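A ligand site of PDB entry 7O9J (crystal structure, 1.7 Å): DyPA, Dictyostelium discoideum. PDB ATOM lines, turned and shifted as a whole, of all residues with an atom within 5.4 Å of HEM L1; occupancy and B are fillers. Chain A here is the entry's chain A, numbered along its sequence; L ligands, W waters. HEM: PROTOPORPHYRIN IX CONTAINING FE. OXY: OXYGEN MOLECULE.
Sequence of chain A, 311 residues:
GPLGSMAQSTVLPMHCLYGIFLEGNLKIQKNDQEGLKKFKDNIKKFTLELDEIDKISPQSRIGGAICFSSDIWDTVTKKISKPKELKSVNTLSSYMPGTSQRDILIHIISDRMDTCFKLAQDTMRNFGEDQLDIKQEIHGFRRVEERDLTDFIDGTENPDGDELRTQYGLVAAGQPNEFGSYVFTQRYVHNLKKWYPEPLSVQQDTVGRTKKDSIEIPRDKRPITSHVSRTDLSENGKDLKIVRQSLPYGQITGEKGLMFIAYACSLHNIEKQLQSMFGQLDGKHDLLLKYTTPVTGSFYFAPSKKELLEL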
ATOM      1  N   ASP A 148      30.233 -17.035 -16.874  1.00  0.00           N
ATOM      2  CA  ASP A 148      30.909 -17.700 -17.986  1.00  0.00           C
ATOM      3  C   ASP A 148      32.197 -18.341 -17.457  1.00  0.00           C
ATOM      4  O   ASP A 148      32.672 -18.011 -16.375  1.00  0.00           O
ATOM      5  CB  ASP A 148      31.203 -16.666 -19.085  1.00  0.00           C
ATOM      6  CG  ASP A 148      32.117 -17.195 -20.176  1.00  0.00           C
ATOM      7  OD1 ASP A 148      31.606 -17.885 -21.083  1.00  0.00           O
ATOM      8  OD2 ASP A 148      33.322 -16.887 -20.147  1.00  0.00           O
ATOM      9  N   THR A 150      35.151 -17.757 -18.200  1.00  0.00           N
ATOM     10  CA  THR A 150      36.110 -16.722 -17.825  1.00  0.00           C
ATOM     11  C   THR A 150      35.962 -16.290 -16.375  1.00  0.00           C
ATOM     12  O   THR A 150      36.806 -15.531 -15.863  1.00  0.00           O
ATOM     13  CB  THR A 150      35.943 -15.477 -18.678  1.00  0.00           C
ATOM     14  OG1 THR A 150      34.595 -14.999 -18.551  1.00  0.00           O
ATOM     15  CG2 THR A 150      36.313 -15.740 -20.137  1.00  0.00           C
ATOM     16  N   PHE A 152      33.645 -14.328 -15.318  1.00  0.00           N
ATOM     17  CA  PHE A 152      32.847 -13.107 -15.295  1.00  0.00           C
ATOM     18  C   PHE A 152      31.358 -13.441 -15.397  1.00  0.00           C
ATOM     19  O   PHE A 152      30.975 -14.364 -16.129  1.00  0.00           O
ATOM     20  CB  PHE A 152      33.236 -12.172 -16.452  1.00  0.00           C
ATOM     21  CG  PHE A 152      34.460 -11.354 -16.172  1.00  0.00           C
ATOM     22  CD1 PHE A 152      35.705 -11.978 -16.058  1.00  0.00           C
ATOM     23  CD2 PHE A 152      34.377  -9.977 -15.997  1.00  0.00           C
ATOM     24  CE1 PHE A 152      36.851 -11.230 -15.771  1.00  0.00           C
ATOM     25  CE2 PHE A 152      35.529  -9.218 -15.729  1.00  0.00           C
ATOM     26  CZ  PHE A 152      36.764  -9.856 -15.604  1.00  0.00           C
ATOM     27  N   ILE A 153      30.527 -12.696 -14.664  1.00  0.00           N
ATOM     28  CA  ILE A 153      29.079 -12.827 -14.802  1.00  0.00           C
ATOM     29  C   ILE A 153      28.676 -12.503 -16.230  1.00  0.00           C
ATOM     30  O   ILE A 153      29.102 -11.485 -16.790  1.00  0.00           O
ATOM     31  CB  ILE A 153      28.363 -11.906 -13.808  1.00  0.00           C
ATOM     32  CG1 ILE A 153      28.691 -12.295 -12.365  1.00  0.00           C
ATOM     33  CG2 ILE A 153      26.842 -11.923 -14.035  1.00  0.00           C
ATOM     34  CD1 ILE A 153      28.276 -11.220 -11.362  1.00  0.00           C
ATOM     35  N   ASP A 154      27.862 -13.372 -16.839  1.00  0.00           N
ATOM     36  CA  ASP A 154      27.356 -13.171 -18.201  1.00  0.00           C
ATOM     37  C   ASP A 154      25.860 -12.907 -18.114  1.00  0.00           C
ATOM     38  O   ASP A 154      25.110 -13.771 -17.653  1.00  0.00           O
ATOM     39  CB  ASP A 154      27.634 -14.403 -19.084  1.00  0.00           C
ATOM     40  CG  ASP A 154      27.211 -14.211 -20.551  1.00  0.00           C
ATOM     41  OD1 ASP A 154      27.200 -13.060 -21.042  1.00  0.00           O
ATOM     42  OD2 ASP A 154      26.891 -15.225 -21.213  1.00  0.00           O
ATOM     43  N   GLY A 155      25.433 -11.723 -18.550  1.00  0.00           N
ATOM     44  CA  GLY A 155      24.015 -11.407 -18.604  1.00  0.00           C
ATOM     45  C   GLY A 155      23.620 -10.060 -18.003  1.00  0.00           C
ATOM     46  O   GLY A 155      22.460  -9.648 -18.145  1.00  0.00           O
ATOM     47  N   THR A 156      24.571  -9.375 -17.375  1.00  0.00           N
ATOM     48  CA  THR A 156      24.256  -8.177 -16.590  1.00  0.00           C
ATOM     49  C   THR A 156      23.413  -7.167 -17.376  1.00  0.00           C
ATOM     50  O   THR A 156      22.420  -6.646 -16.861  1.00  0.00           O
ATOM     51  CB  THR A 156      25.546  -7.516 -16.093  1.00  0.00           C
ATOM     52  OG1 THR A 156      26.270  -8.481 -15.320  1.00  0.00           O
ATOM     53  CG2 THR A 156      25.239  -6.302 -15.225  1.00  0.00           C
ATOM     54  N   GLU A 157      23.791  -6.881 -18.620  1.00  0.00           N
ATOM     55  CA  GLU A 157      23.078  -5.882 -19.413  1.00  0.00           C
ATOM     56  C   GLU A 157      22.079  -6.483 -20.411  1.00  0.00           C
ATOM     57  O   GLU A 157      21.595  -5.764 -21.302  1.00  0.00           O
ATOM     58  CB  GLU A 157      24.073  -4.966 -20.126  1.00  0.00           C
ATOM     59  CG  GLU A 157      24.868  -4.053 -19.173  1.00  0.00           C
ATOM     60  CD  GLU A 157      23.967  -3.094 -18.396  1.00  0.00           C
ATOM     61  OE1 GLU A 157      22.986  -2.577 -18.973  1.00  0.00           O
ATOM     62  OE2 GLU A 157      24.252  -2.858 -17.198  1.00  0.00           O
ATOM     63  N   ASN A 158      21.769  -7.764 -20.297  1.00  0.00           N
ATOM     64  CA  ASN A 158      20.658  -8.328 -21.047  1.00  0.00           C
ATOM     65  C   ASN A 158      19.380  -7.542 -20.734  1.00  0.00           C
ATOM     66  O   ASN A 158      19.132  -7.218 -19.557  1.00  0.00           O
ATOM     67  CB  ASN A 158      20.440  -9.789 -20.647  1.00  0.00           C
ATOM     68  CG  ASN A 158      20.524 -10.761 -21.805  1.00  0.00           C
ATOM     69  OD1 ASN A 158      20.497 -10.398 -22.983  1.00  0.00           O
ATOM     70  ND2 ASN A 158      20.625 -12.039 -21.453  1.00  0.00           N
ATOM     71  N   PHE A 184      21.037 -16.087 -33.871  1.00  0.00           N
ATOM     72  CA  PHE A 184      22.422 -16.359 -34.224  1.00  0.00           C
ATOM     73  C   PHE A 184      22.995 -17.293 -33.172  1.00  0.00           C
ATOM     74  O   PHE A 184      22.894 -17.012 -31.972  1.00  0.00           O
ATOM     75  CB  PHE A 184      23.230 -15.053 -34.279  1.00  0.00           C
ATOM     76  CG  PHE A 184      24.731 -15.240 -34.414  1.00  0.00           C
ATOM     77  CD1 PHE A 184      25.275 -15.861 -35.534  1.00  0.00           C
ATOM     78  CD2 PHE A 184      25.596 -14.759 -33.432  1.00  0.00           C
ATOM     79  CE1 PHE A 184      26.642 -16.023 -35.666  1.00  0.00           C
ATOM     80  CE2 PHE A 184      26.968 -14.915 -33.570  1.00  0.00           C
ATOM     81  CZ  PHE A 184      27.495 -15.540 -34.693  1.00  0.00           C
ATOM     82  N   GLN A 186      26.598 -19.545 -32.068  1.00  0.00           N
ATOM     83  CA  GLN A 186      28.043 -19.564 -32.299  1.00  0.00           C
ATOM     84  C   GLN A 186      28.702 -20.259 -31.120  1.00  0.00           C
ATOM     85  O   GLN A 186      28.651 -19.743 -29.999  1.00  0.00           O
ATOM     86  CB  GLN A 186      28.566 -18.135 -32.458  1.00  0.00           C
ATOM     87  CG  GLN A 186      30.034 -18.011 -32.821  1.00  0.00           C
ATOM     88  CD  GLN A 186      30.403 -16.572 -33.186  1.00  0.00           C
ATOM     89  OE1 GLN A 186      30.080 -15.639 -32.435  1.00  0.00           O
ATOM     90  NE2 GLN A 186      31.039 -16.379 -34.328  1.00  0.00           N
ATOM     91  N   TYR A 188      31.835 -21.223 -28.953  1.00  0.00           N
ATOM     92  CA  TYR A 188      33.181 -20.758 -28.643  1.00  0.00           C
ATOM     93  C   TYR A 188      33.934 -21.831 -27.871  1.00  0.00           C
ATOM     94  O   TYR A 188      33.373 -22.495 -26.992  1.00  0.00           O
ATOM     95  CB  TYR A 188      33.145 -19.470 -27.823  1.00  0.00           C
ATOM     96  CG  TYR A 188      32.886 -18.248 -28.659  1.00  0.00           C
ATOM     97  CD1 TYR A 188      31.583 -17.879 -28.990  1.00  0.00           C
ATOM     98  CD2 TYR A 188      33.946 -17.461 -29.120  1.00  0.00           C
ATOM     99  CE1 TYR A 188      31.344 -16.735 -29.778  1.00  0.00           C
ATOM    100  CE2 TYR A 188      33.721 -16.332 -29.895  1.00  0.00           C
ATOM    101  CZ  TYR A 188      32.425 -15.989 -30.217  1.00  0.00           C
ATOM    102  OH  TYR A 188      32.204 -14.870 -31.002  1.00  0.00           O
ATOM    103  N   HIS A 190      37.040 -21.908 -25.326  1.00  0.00           N
ATOM    104  CA  HIS A 190      37.864 -21.038 -24.498  1.00  0.00           C
ATOM    105  C   HIS A 190      39.274 -21.604 -24.342  1.00  0.00           C
ATOM    106  O   HIS A 190      39.452 -22.820 -24.217  1.00  0.00           O
ATOM    107  CB  HIS A 190      37.267 -20.861 -23.099  1.00  0.00           C
ATOM    108  CG  HIS A 190      36.040 -19.992 -23.046  1.00  0.00           C
ATOM    109  ND1 HIS A 190      35.381 -19.547 -24.175  1.00  0.00           N
ATOM    110  CD2 HIS A 190      35.347 -19.503 -21.990  1.00  0.00           C
ATOM    111  CE1 HIS A 190      34.351 -18.810 -23.809  1.00  0.00           C
ATOM    112  NE2 HIS A 190      34.303 -18.769 -22.493  1.00  0.00           N
ATOM    113  N   VAL A 207      37.149  -7.381 -20.634  1.00  0.00           N
ATOM    114  CA  VAL A 207      35.695  -7.487 -20.651  1.00  0.00           C
ATOM    115  C   VAL A 207      35.050  -6.103 -20.651  1.00  0.00           C
ATOM    116  O   VAL A 207      34.104  -5.841 -21.415  1.00  0.00           O
ATOM    117  CB  VAL A 207      35.208  -8.325 -19.457  1.00  0.00           C
ATOM    118  CG1 VAL A 207      33.696  -8.321 -19.402  1.00  0.00           C
ATOM    119  CG2 VAL A 207      35.763  -9.747 -19.554  1.00  0.00           C
ATOM    120  N   ARG A 209      34.037  -4.692 -17.491  1.00  0.00           N
ATOM    121  CA  ARG A 209      33.306  -4.633 -16.240  1.00  0.00           C
ATOM    122  C   ARG A 209      34.183  -5.235 -15.152  1.00  0.00           C
ATOM    123  O   ARG A 209      35.135  -5.966 -15.450  1.00  0.00           O
ATOM    124  CB  ARG A 209      31.962  -5.388 -16.304  1.00  0.00           C
ATOM    125  CG  ARG A 209      31.174  -5.147 -17.592  1.00  0.00           C
ATOM    126  CD  ARG A 209      29.789  -5.806 -17.550  1.00  0.00           C
ATOM    127  NE  ARG A 209      28.943  -5.147 -16.547  1.00  0.00           N
ATOM    128  CZ  ARG A 209      28.192  -4.074 -16.787  1.00  0.00           C
ATOM    129  NH1 ARG A 209      28.127  -3.544 -18.009  1.00  0.00           N
ATOM    130  NH2 ARG A 209      27.499  -3.529 -15.791  1.00  0.00           N
ATOM    131  N   SER A 214      30.491  -7.225 -11.562  1.00  0.00           N
ATOM    132  CA  SER A 214      30.034  -6.819 -12.895  1.00  0.00           C
ATOM    133  C   SER A 214      29.618  -5.350 -12.929  1.00  0.00           C
ATOM    134  O   SER A 214      28.616  -4.982 -13.550  1.00  0.00           O
ATOM    135  CB  SER A 214      28.895  -7.725 -13.399  1.00  0.00           C
ATOM    136  OG  SER A 214      28.783  -7.632 -14.821  1.00  0.00           O
ATOM    137  N   HIS A 227      35.320  -5.818 -24.531  1.00  0.00           N
ATOM    138  CA  HIS A 227      34.148  -6.486 -25.078  1.00  0.00           C
ATOM    139  C   HIS A 227      32.896  -5.605 -24.995  1.00  0.00           C
ATOM    140  O   HIS A 227      32.149  -5.500 -25.970  1.00  0.00           O
ATOM    141  CB  HIS A 227      33.944  -7.811 -24.353  1.00  0.00           C
ATOM    142  CG  HIS A 227      32.814  -8.619 -24.893  1.00  0.00           C
ATOM    143  ND1 HIS A 227      32.742  -8.990 -26.223  1.00  0.00           N
ATOM    144  CD2 HIS A 227      31.709  -9.110 -24.294  1.00  0.00           C
ATOM    145  CE1 HIS A 227      31.647  -9.687 -26.414  1.00  0.00           C
ATOM    146  NE2 HIS A 227      30.999  -9.768 -25.268  1.00  0.00           N
ATOM    147  N   VAL A 228      32.695  -4.925 -23.856  1.00  0.00           N
ATOM    148  CA  VAL A 228      31.538  -4.044 -23.722  1.00  0.00           C
ATOM    149  C   VAL A 228      31.605  -2.886 -24.736  1.00  0.00           C
ATOM    150  O   VAL A 228      30.583  -2.516 -25.336  1.00  0.00           O
ATOM    151  CB  VAL A 228      31.413  -3.517 -22.277  1.00  0.00           C
ATOM    152  CG1 VAL A 228      30.340  -2.441 -22.207  1.00  0.00           C
ATOM    153  CG2 VAL A 228      31.074  -4.687 -21.323  1.00  0.00           C
ATOM    154  N   THR A 231      30.442  -4.188 -28.131  1.00  0.00           N
ATOM    155  CA  THR A 231      29.082  -4.689 -28.312  1.00  0.00           C
ATOM    156  C   THR A 231      27.982  -3.726 -27.885  1.00  0.00           C
ATOM    157  O   THR A 231      26.822  -3.949 -28.255  1.00  0.00           O
ATOM    158  CB  THR A 231      28.880  -6.016 -27.551  1.00  0.00           C
ATOM    159  OG1 THR A 231      29.179  -5.820 -26.164  1.00  0.00           O
ATOM    160  CG2 THR A 231      29.778  -7.119 -28.122  1.00  0.00           C
ATOM    161  N   ASP A 232      28.297  -2.683 -27.115  1.00  0.00           N
ATOM    162  CA  ASP A 232      27.312  -1.686 -26.708  1.00  0.00           C
ATOM    163  C   ASP A 232      27.267  -0.600 -27.770  1.00  0.00           C
ATOM    164  O   ASP A 232      27.948   0.428 -27.680  1.00  0.00           O
ATOM    165  CB  ASP A 232      27.660  -1.136 -25.322  1.00  0.00           C
ATOM    166  CG  ASP A 232      26.709  -0.055 -24.848  1.00  0.00           C
ATOM    167  OD1 ASP A 232      25.608   0.100 -25.424  1.00  0.00           O
ATOM    168  OD2 ASP A 232      27.067   0.660 -23.882  1.00  0.00           O
ATOM    169  N   LYS A 241      20.243  -3.287 -29.179  1.00  0.00           N
ATOM    170  CA  LYS A 241      20.253  -4.315 -28.150  1.00  0.00           C
ATOM    171  C   LYS A 241      19.760  -5.659 -28.705  1.00  0.00           C
ATOM    172  O   LYS A 241      19.018  -5.725 -29.690  1.00  0.00           O
ATOM    173  CB  LYS A 241      19.404  -3.880 -26.952  1.00  0.00           C
ATOM    174  CG  LYS A 241      19.955  -2.626 -26.253  1.00  0.00           C
ATOM    175  CD  LYS A 241      19.221  -2.333 -24.961  1.00  0.00           C
ATOM    176  CE  LYS A 241      19.872  -1.188 -24.200  1.00  0.00           C
ATOM    177  NZ  LYS A 241      21.261  -1.524 -23.781  1.00  0.00           N
ATOM    178  N   ILE A 242      20.175  -6.744 -28.036  1.00  0.00           N
ATOM    179  CA  ILE A 242      19.805  -8.101 -28.416  1.00  0.00           C
ATOM    180  C   ILE A 242      19.482  -8.856 -27.132  1.00  0.00           C
ATOM    181  O   ILE A 242      19.755  -8.396 -26.028  1.00  0.00           O
ATOM    182  CB  ILE A 242      20.941  -8.810 -29.197  1.00  0.00           C
ATOM    183  CG1 ILE A 242      22.198  -8.870 -28.331  1.00  0.00           C
ATOM    184  CG2 ILE A 242      21.257  -8.059 -30.512  1.00  0.00           C
ATOM    185  CD1 ILE A 242      23.364  -9.622 -28.988  1.00  0.00           C
ATOM    186  N   ARG A 244      20.248 -12.309 -25.244  1.00  0.00           N
ATOM    187  CA  ARG A 244      21.170 -13.441 -25.244  1.00  0.00           C
ATOM    188  C   ARG A 244      20.657 -14.549 -24.334  1.00  0.00           C
ATOM    189  O   ARG A 244      20.144 -14.275 -23.241  1.00  0.00           O
ATOM    190  CB  ARG A 244      22.567 -13.008 -24.814  1.00  0.00           C
ATOM    191  CG  ARG A 244      23.274 -12.079 -25.816  1.00  0.00           C
ATOM    192  CD  ARG A 244      24.506 -11.426 -25.195  1.00  0.00           C
ATOM    193  NE  ARG A 244      24.131 -10.392 -24.228  1.00  0.00           N
ATOM    194  CZ  ARG A 244      24.696 -10.205 -23.040  1.00  0.00           C
ATOM    195  NH1 ARG A 244      25.689 -10.994 -22.620  1.00  0.00           N
ATOM    196  NH2 ARG A 244      24.250  -9.239 -22.247  1.00  0.00           N
ATOM    197  N   LEU A 258      31.690 -21.347 -24.348  1.00  0.00           N
ATOM    198  CA  LEU A 258      30.384 -20.728 -24.279  1.00  0.00           C
ATOM    199  C   LEU A 258      29.608 -21.110 -25.522  1.00  0.00           C
ATOM    200  O   LEU A 258      30.101 -20.939 -26.637  1.00  0.00           O
ATOM    201  CB  LEU A 258      30.482 -19.190 -24.198  1.00  0.00           C
ATOM    202  CG  LEU A 258      29.121 -18.486 -24.071  1.00  0.00           C
ATOM    203  CD1 LEU A 258      28.522 -18.746 -22.679  1.00  0.00           C
ATOM    204  CD2 LEU A 258      29.249 -16.995 -24.326  1.00  0.00           C
ATOM    205  N   PHE A 260      27.111 -19.624 -27.509  1.00  0.00           N
ATOM    206  CA  PHE A 260      26.474 -18.322 -27.666  1.00  0.00           C
ATOM    207  C   PHE A 260      25.193 -18.444 -28.488  1.00  0.00           C
ATOM    208  O   PHE A 260      25.171 -19.077 -29.547  1.00  0.00           O
ATOM    209  CB  PHE A 260      27.411 -17.322 -28.342  1.00  0.00           C
ATOM    210  CG  PHE A 260      26.833 -15.936 -28.445  1.00  0.00           C
ATOM    211  CD1 PHE A 260      27.009 -15.041 -27.393  1.00  0.00           C
ATOM    212  CD2 PHE A 260      26.073 -15.556 -29.546  1.00  0.00           C
ATOM    213  CE1 PHE A 260      26.453 -13.779 -27.450  1.00  0.00           C
ATOM    214  CE2 PHE A 260      25.520 -14.304 -29.612  1.00  0.00           C
ATOM    215  CZ  PHE A 260      25.713 -13.405 -28.558  1.00  0.00           C
ATOM    216  N   ILE A 270      22.471  -7.847 -34.479  1.00  0.00           N
ATOM    217  CA  ILE A 270      23.496  -8.864 -34.233  1.00  0.00           C
ATOM    218  C   ILE A 270      24.681  -8.651 -35.160  1.00  0.00           C
ATOM    219  O   ILE A 270      25.833  -8.657 -34.720  1.00  0.00           O
ATOM    220  CB  ILE A 270      22.902 -10.270 -34.432  1.00  0.00           C
ATOM    221  CG1 ILE A 270      21.737 -10.511 -33.467  1.00  0.00           C
ATOM    222  CG2 ILE A 270      23.991 -11.344 -34.238  1.00  0.00           C
ATOM    223  CD1 ILE A 270      20.961 -11.794 -33.769  1.00  0.00           C
ATOM    224  N   GLN A 273      27.245  -5.976 -34.378  1.00  0.00           N
ATOM    225  CA  GLN A 273      28.139  -6.333 -33.276  1.00  0.00           C
ATOM    226  C   GLN A 273      29.216  -7.302 -33.750  1.00  0.00           C
ATOM    227  O   GLN A 273      30.370  -7.228 -33.298  1.00  0.00           O
ATOM    228  CB  GLN A 273      27.335  -6.918 -32.121  1.00  0.00           C
ATOM    229  CG  GLN A 273      26.373  -5.919 -31.500  1.00  0.00           C
ATOM    230  CD  GLN A 273      25.638  -6.503 -30.318  1.00  0.00           C
ATOM    231  OE1 GLN A 273      26.191  -7.323 -29.591  1.00  0.00           O
ATOM    232  NE2 GLN A 273      24.388  -6.088 -30.125  1.00  0.00           N
ATOM    233  N   LEU A 274      28.874  -8.215 -34.659  1.00  0.00           N
ATOM    234  CA  LEU A 274      29.879  -9.119 -35.211  1.00  0.00           C
ATOM    235  C   LEU A 274      30.904  -8.360 -36.045  1.00  0.00           C
ATOM    236  O   LEU A 274      32.110  -8.654 -35.988  1.00  0.00           O
ATOM    237  CB  LEU A 274      29.220 -10.216 -36.050  1.00  0.00           C
ATOM    238  CG  LEU A 274      28.267 -11.121 -35.265  1.00  0.00           C
ATOM    239  CD1 LEU A 274      27.623 -12.082 -36.253  1.00  0.00           C
ATOM    240  CD2 LEU A 274      28.993 -11.870 -34.151  1.00  0.00           C
ATOM    241  N   MET A 277      33.177  -6.753 -33.394  1.00  0.00           N
ATOM    242  CA  MET A 277      34.054  -7.665 -32.655  1.00  0.00           C
ATOM    243  C   MET A 277      35.162  -8.235 -33.543  1.00  0.00           C
ATOM    244  O   MET A 277      36.287  -8.440 -33.086  1.00  0.00           O
ATOM    245  CB  MET A 277      33.251  -8.811 -32.046  1.00  0.00           C
ATOM    246  CG  MET A 277      32.338  -8.402 -30.902  1.00  0.00           C
ATOM    247  SD  MET A 277      31.351  -9.821 -30.349  1.00  0.00           S
ATOM    248  CE  MET A 277      32.625 -11.002 -29.896  1.00  0.00           C
ATOM    249  N   LEU A 288      38.487  -9.965 -26.144  1.00  0.00           N
ATOM    250  CA  LEU A 288      38.088 -11.304 -25.715  1.00  0.00           C
ATOM    251  C   LEU A 288      38.591 -12.369 -26.679  1.00  0.00           C
ATOM    252  O   LEU A 288      38.850 -13.505 -26.260  1.00  0.00           O
ATOM    253  CB  LEU A 288      36.568 -11.399 -25.589  1.00  0.00           C
ATOM    254  CG  LEU A 288      35.888 -11.516 -24.236  1.00  0.00           C
ATOM    255  CD1 LEU A 288      34.441 -11.892 -24.468  1.00  0.00           C
ATOM    256  CD2 LEU A 288      36.579 -12.510 -23.305  1.00  0.00           C
ATOM    257  N   THR A 292      39.508 -16.850 -26.737  1.00  0.00           N
ATOM    258  CA  THR A 292      38.451 -17.782 -27.124  1.00  0.00           C
ATOM    259  C   THR A 292      38.282 -17.701 -28.634  1.00  0.00           C
ATOM    260  O   THR A 292      38.630 -16.692 -29.260  1.00  0.00           O
ATOM    261  CB  THR A 292      37.150 -17.471 -26.377  1.00  0.00           C
ATOM    262  OG1 THR A 292      36.171 -18.457 -26.706  1.00  0.00           O
ATOM    263  CG2 THR A 292      36.628 -16.089 -26.775  1.00  0.00           C
HETATM  264  CHA HEM L   1      28.218  -8.531 -22.545  1.00  0.00           C
HETATM  265  CHB HEM L   1      30.907 -12.578 -22.258  1.00  0.00           C
HETATM  266  CHC HEM L   1      30.352 -13.228 -27.091  1.00  0.00           C
HETATM  267  CHD HEM L   1      27.148  -9.583 -27.192  1.00  0.00           C
HETATM  268  C1A HEM L   1      29.028  -9.555 -22.092  1.00  0.00           C
HETATM  269  C2A HEM L   1      29.555  -9.612 -20.768  1.00  0.00           C
HETATM  270  C3A HEM L   1      30.303 -10.748 -20.687  1.00  0.00           C
HETATM  271  C4A HEM L   1      30.243 -11.404 -21.944  1.00  0.00           C
HETATM  272  CMA HEM L   1      31.065 -11.252 -19.484  1.00  0.00           C
HETATM  273  CAA HEM L   1      29.333  -8.600 -19.647  1.00  0.00           C
HETATM  274  CBA HEM L   1      28.094  -8.888 -18.794  1.00  0.00           C
HETATM  275  CGA HEM L   1      26.813  -8.615 -19.553  1.00  0.00           C
HETATM  276  O1A HEM L   1      26.335  -7.455 -19.672  1.00  0.00           O
HETATM  277  O2A HEM L   1      26.204  -9.575 -20.072  1.00  0.00           O
HETATM  278  C1B HEM L   1      30.987 -13.082 -23.563  1.00  0.00           C
HETATM  279  C2B HEM L   1      31.761 -14.226 -23.905  1.00  0.00           C
HETATM  280  C3B HEM L   1      31.612 -14.431 -25.261  1.00  0.00           C
HETATM  281  C4B HEM L   1      30.725 -13.355 -25.737  1.00  0.00           C
HETATM  282  CMB HEM L   1      32.563 -15.041 -22.902  1.00  0.00           C
HETATM  283  CAB HEM L   1      32.188 -15.483 -26.122  1.00  0.00           C
HETATM  284  CBB HEM L   1      33.317 -16.132 -25.826  1.00  0.00           C
HETATM  285  C1C HEM L   1      29.420 -12.308 -27.549  1.00  0.00           C
HETATM  286  C2C HEM L   1      28.999 -12.165 -28.889  1.00  0.00           C
HETATM  287  C3C HEM L   1      28.069 -11.121 -28.918  1.00  0.00           C
HETATM  288  C4C HEM L   1      27.973 -10.624 -27.579  1.00  0.00           C
HETATM  289  CMC HEM L   1      29.456 -13.055 -30.028  1.00  0.00           C
HETATM  290  CAC HEM L   1      27.312 -10.538 -30.051  1.00  0.00           C
HETATM  291  CBC HEM L   1      26.944 -11.182 -31.162  1.00  0.00           C
HETATM  292  C1D HEM L   1      27.223  -9.042 -25.903  1.00  0.00           C
HETATM  293  C2D HEM L   1      26.393  -7.872 -25.559  1.00  0.00           C
HETATM  294  C3D HEM L   1      26.695  -7.561 -24.283  1.00  0.00           C
HETATM  295  C4D HEM L   1      27.692  -8.557 -23.845  1.00  0.00           C
HETATM  296  CMD HEM L   1      25.412  -7.133 -26.471  1.00  0.00           C
HETATM  297  CAD HEM L   1      26.104  -6.424 -23.477  1.00  0.00           C
HETATM  298  CBD HEM L   1      26.813  -5.106 -23.835  1.00  0.00           C
HETATM  299  CGD HEM L   1      26.198  -3.923 -23.122  1.00  0.00           C
HETATM  300  O1D HEM L   1      25.209  -3.328 -23.623  1.00  0.00           O
HETATM  301  O2D HEM L   1      26.670  -3.516 -22.036  1.00  0.00           O
HETATM  302  NA  HEM L   1      29.507 -10.635 -22.814  1.00  0.00           N
HETATM  303  NB  HEM L   1      30.372 -12.616 -24.662  1.00  0.00           N
HETATM  304  NC  HEM L   1      28.853 -11.331 -26.778  1.00  0.00           N
HETATM  305  ND  HEM L   1      27.946  -9.451 -24.819  1.00  0.00           N
HETATM  306 FE   HEM L   1      29.190 -10.908 -24.774  1.00  0.00          FE
HETATM  307  O1  OXY L   2      26.245 -14.418 -23.974  1.00  0.00           O
HETATM  308  O2  OXY L   2      27.513 -12.531 -24.032  1.00  0.00           O
HETATM  309  O   HOH W   1      22.106  -4.327 -23.505  1.00  0.00           O
HETATM  310  O   HOH W   2      27.837  -5.245 -20.298  1.00  0.00           O
HETATM  311  O   HOH W   3      23.595  -1.455 -21.897  1.00  0.00           O
HETATM  312  O   HOH W   4      24.122  -3.821 -26.285  1.00  0.00           O
HETATM  313  O   HOH W   5      26.550  -1.040 -21.099  1.00  0.00           O
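Asp 148 touches HEM L1. Phe 152 touches HEM L1 (CB to CMA, 3.8 Å). O of Ile 153 touches CMA of HEM L1 (3.3 Å). Asp 154 touches HEM L1. Gln 186 touches HEM L1. OH of Tyr 188 touches CMC of HEM L1, at 3.4 Å. His 190 touches HEM L1. Val 207 touches HEM L1. Arg 209 touches HEM L1 (CD to CAA, 3.5 Å). Val 228 touches HEM L1. Thr 231 touches HEM L1 (OG1 to CBD, 3.4 Å). Asp 232 touches HEM L1 (CB to O1D, 3.7 Å). CD2 of Leu 258 touches C3B of HEM L1, at 3.6 Å. Phe 260 touches HEM L1. Gln 273 touches HEM L1. Leu 274 touches HEM L1 (CD2 to CBC, 3.7 Å). SD of Met 277 touches C2C of HEM L1 (3.6 Å). CD1 of Leu 288 touches C2B of HEM L1, at 3.6 Å. Thr 292 touches HEM L1 (CG2 to CBB, 3.4 Å). Hydrophobic or aromatic side chains that line HEM L1: Phe 152, Tyr 188, His 190, Val 207, His 227, Val 228, Leu 258, Phe 260, Leu 274, Met 277 and Leu 288. 24 residues have an atom within 4 Å of HEM L1: Asp 148, Phe 152, Ile 153, Asp 154, Gly 155, Thr 156, Glu 157, Gln 186, Tyr 188, His 190, Val 207, Arg 209, His 227, Val 228, Thr 231, Asp 232, Arg 244, Leu 258, Phe 260, Gln 273, Leu 274, Met 277, Leu 288 and Thr 292. The nearest printed residue that does not touch HEM L1 is Ile 242 (4.1 Å).
Water W5 bridges O2D of HEM L1 and OD2 of Asp 232. Water W2 lies within hydrogen-bond range of O2D of HEM L1 (2.7 Å) and NH1 of Arg 209 (2.9 Å). Water W4 lies within hydrogen-bond range of an oxygen (O1D) of HEM L1 (2.9 Å) and the backbone carbonyl oxygen of Thr 231 (3.3 Å). Water W3 lies within hydrogen-bond range of NZ of Lys 241 (3.0 Å), O1D of HEM L1 (3.0 Å) and OE1 of Glu 157 (3.2 Å). Water W1 lies within hydrogen-bond range of O of Glu 157 (2.7 Å), NZ of Lys 241 (2.9 Å) and O1D of HEM L1 (3.3 Å).
The backbone NH (N) of Val 228 is in hydrogen-bond range of the backbone carbonyl oxygen (O) of Val 207, 3.0 Å away. A ring nitrogen (NE2) of His 190 sits at hydrogen-bond distance from the side-chain carboxylate (OD2) of Asp 148. N of His 227 lies within hydrogen-bond range of O of Val 207 (3.3 Å). OG of Ser 214 sits at hydrogen-bond distance from OG1 of Thr 156 (2.7 Å). The backbone carbonyl oxygen (O) of Arg 244 lies within hydrogen-bond range of the side-chain amide nitrogen (ND2) of Asn 158. O of Ser 214 is in hydrogen-bond range of NH2 of Arg 209. ND1 of His 190 is in hydrogen-bond range of OG1 of Thr 292 (2.9 Å). The side-chain hydroxyl of Thr 150 lies close to the backbone NH of Phe 152, 3.4 Å away.
An oxygen (O2A) of HEM L1 is in hydrogen-bond range of the backbone NH (N) of Gly 155, at 2.7 Å. The guanidinium group (NH1) of Arg 244 sits close to an oxygen (O2) of OXY L2 (2.8 Å). An iron atom (FE) of HEM L1 is bound by a ring nitrogen (NE2) of His 227 (2.2 Å). The backbone NH of Glu 157 lies within hydrogen-bond range of an oxygen (O1A) of HEM L1 (2.8 Å). N of Thr 156 lies within hydrogen-bond range of O2A of HEM L1 (3.2 Å). The guanidinium group (NH2) of Arg 244 lies within salt-bridge range of an oxygen (O2A) of HEM L1 (2.9 Å).
An iron atom (FE) of HEM L1 is bound by an oxygen (O2) of OXY L2.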
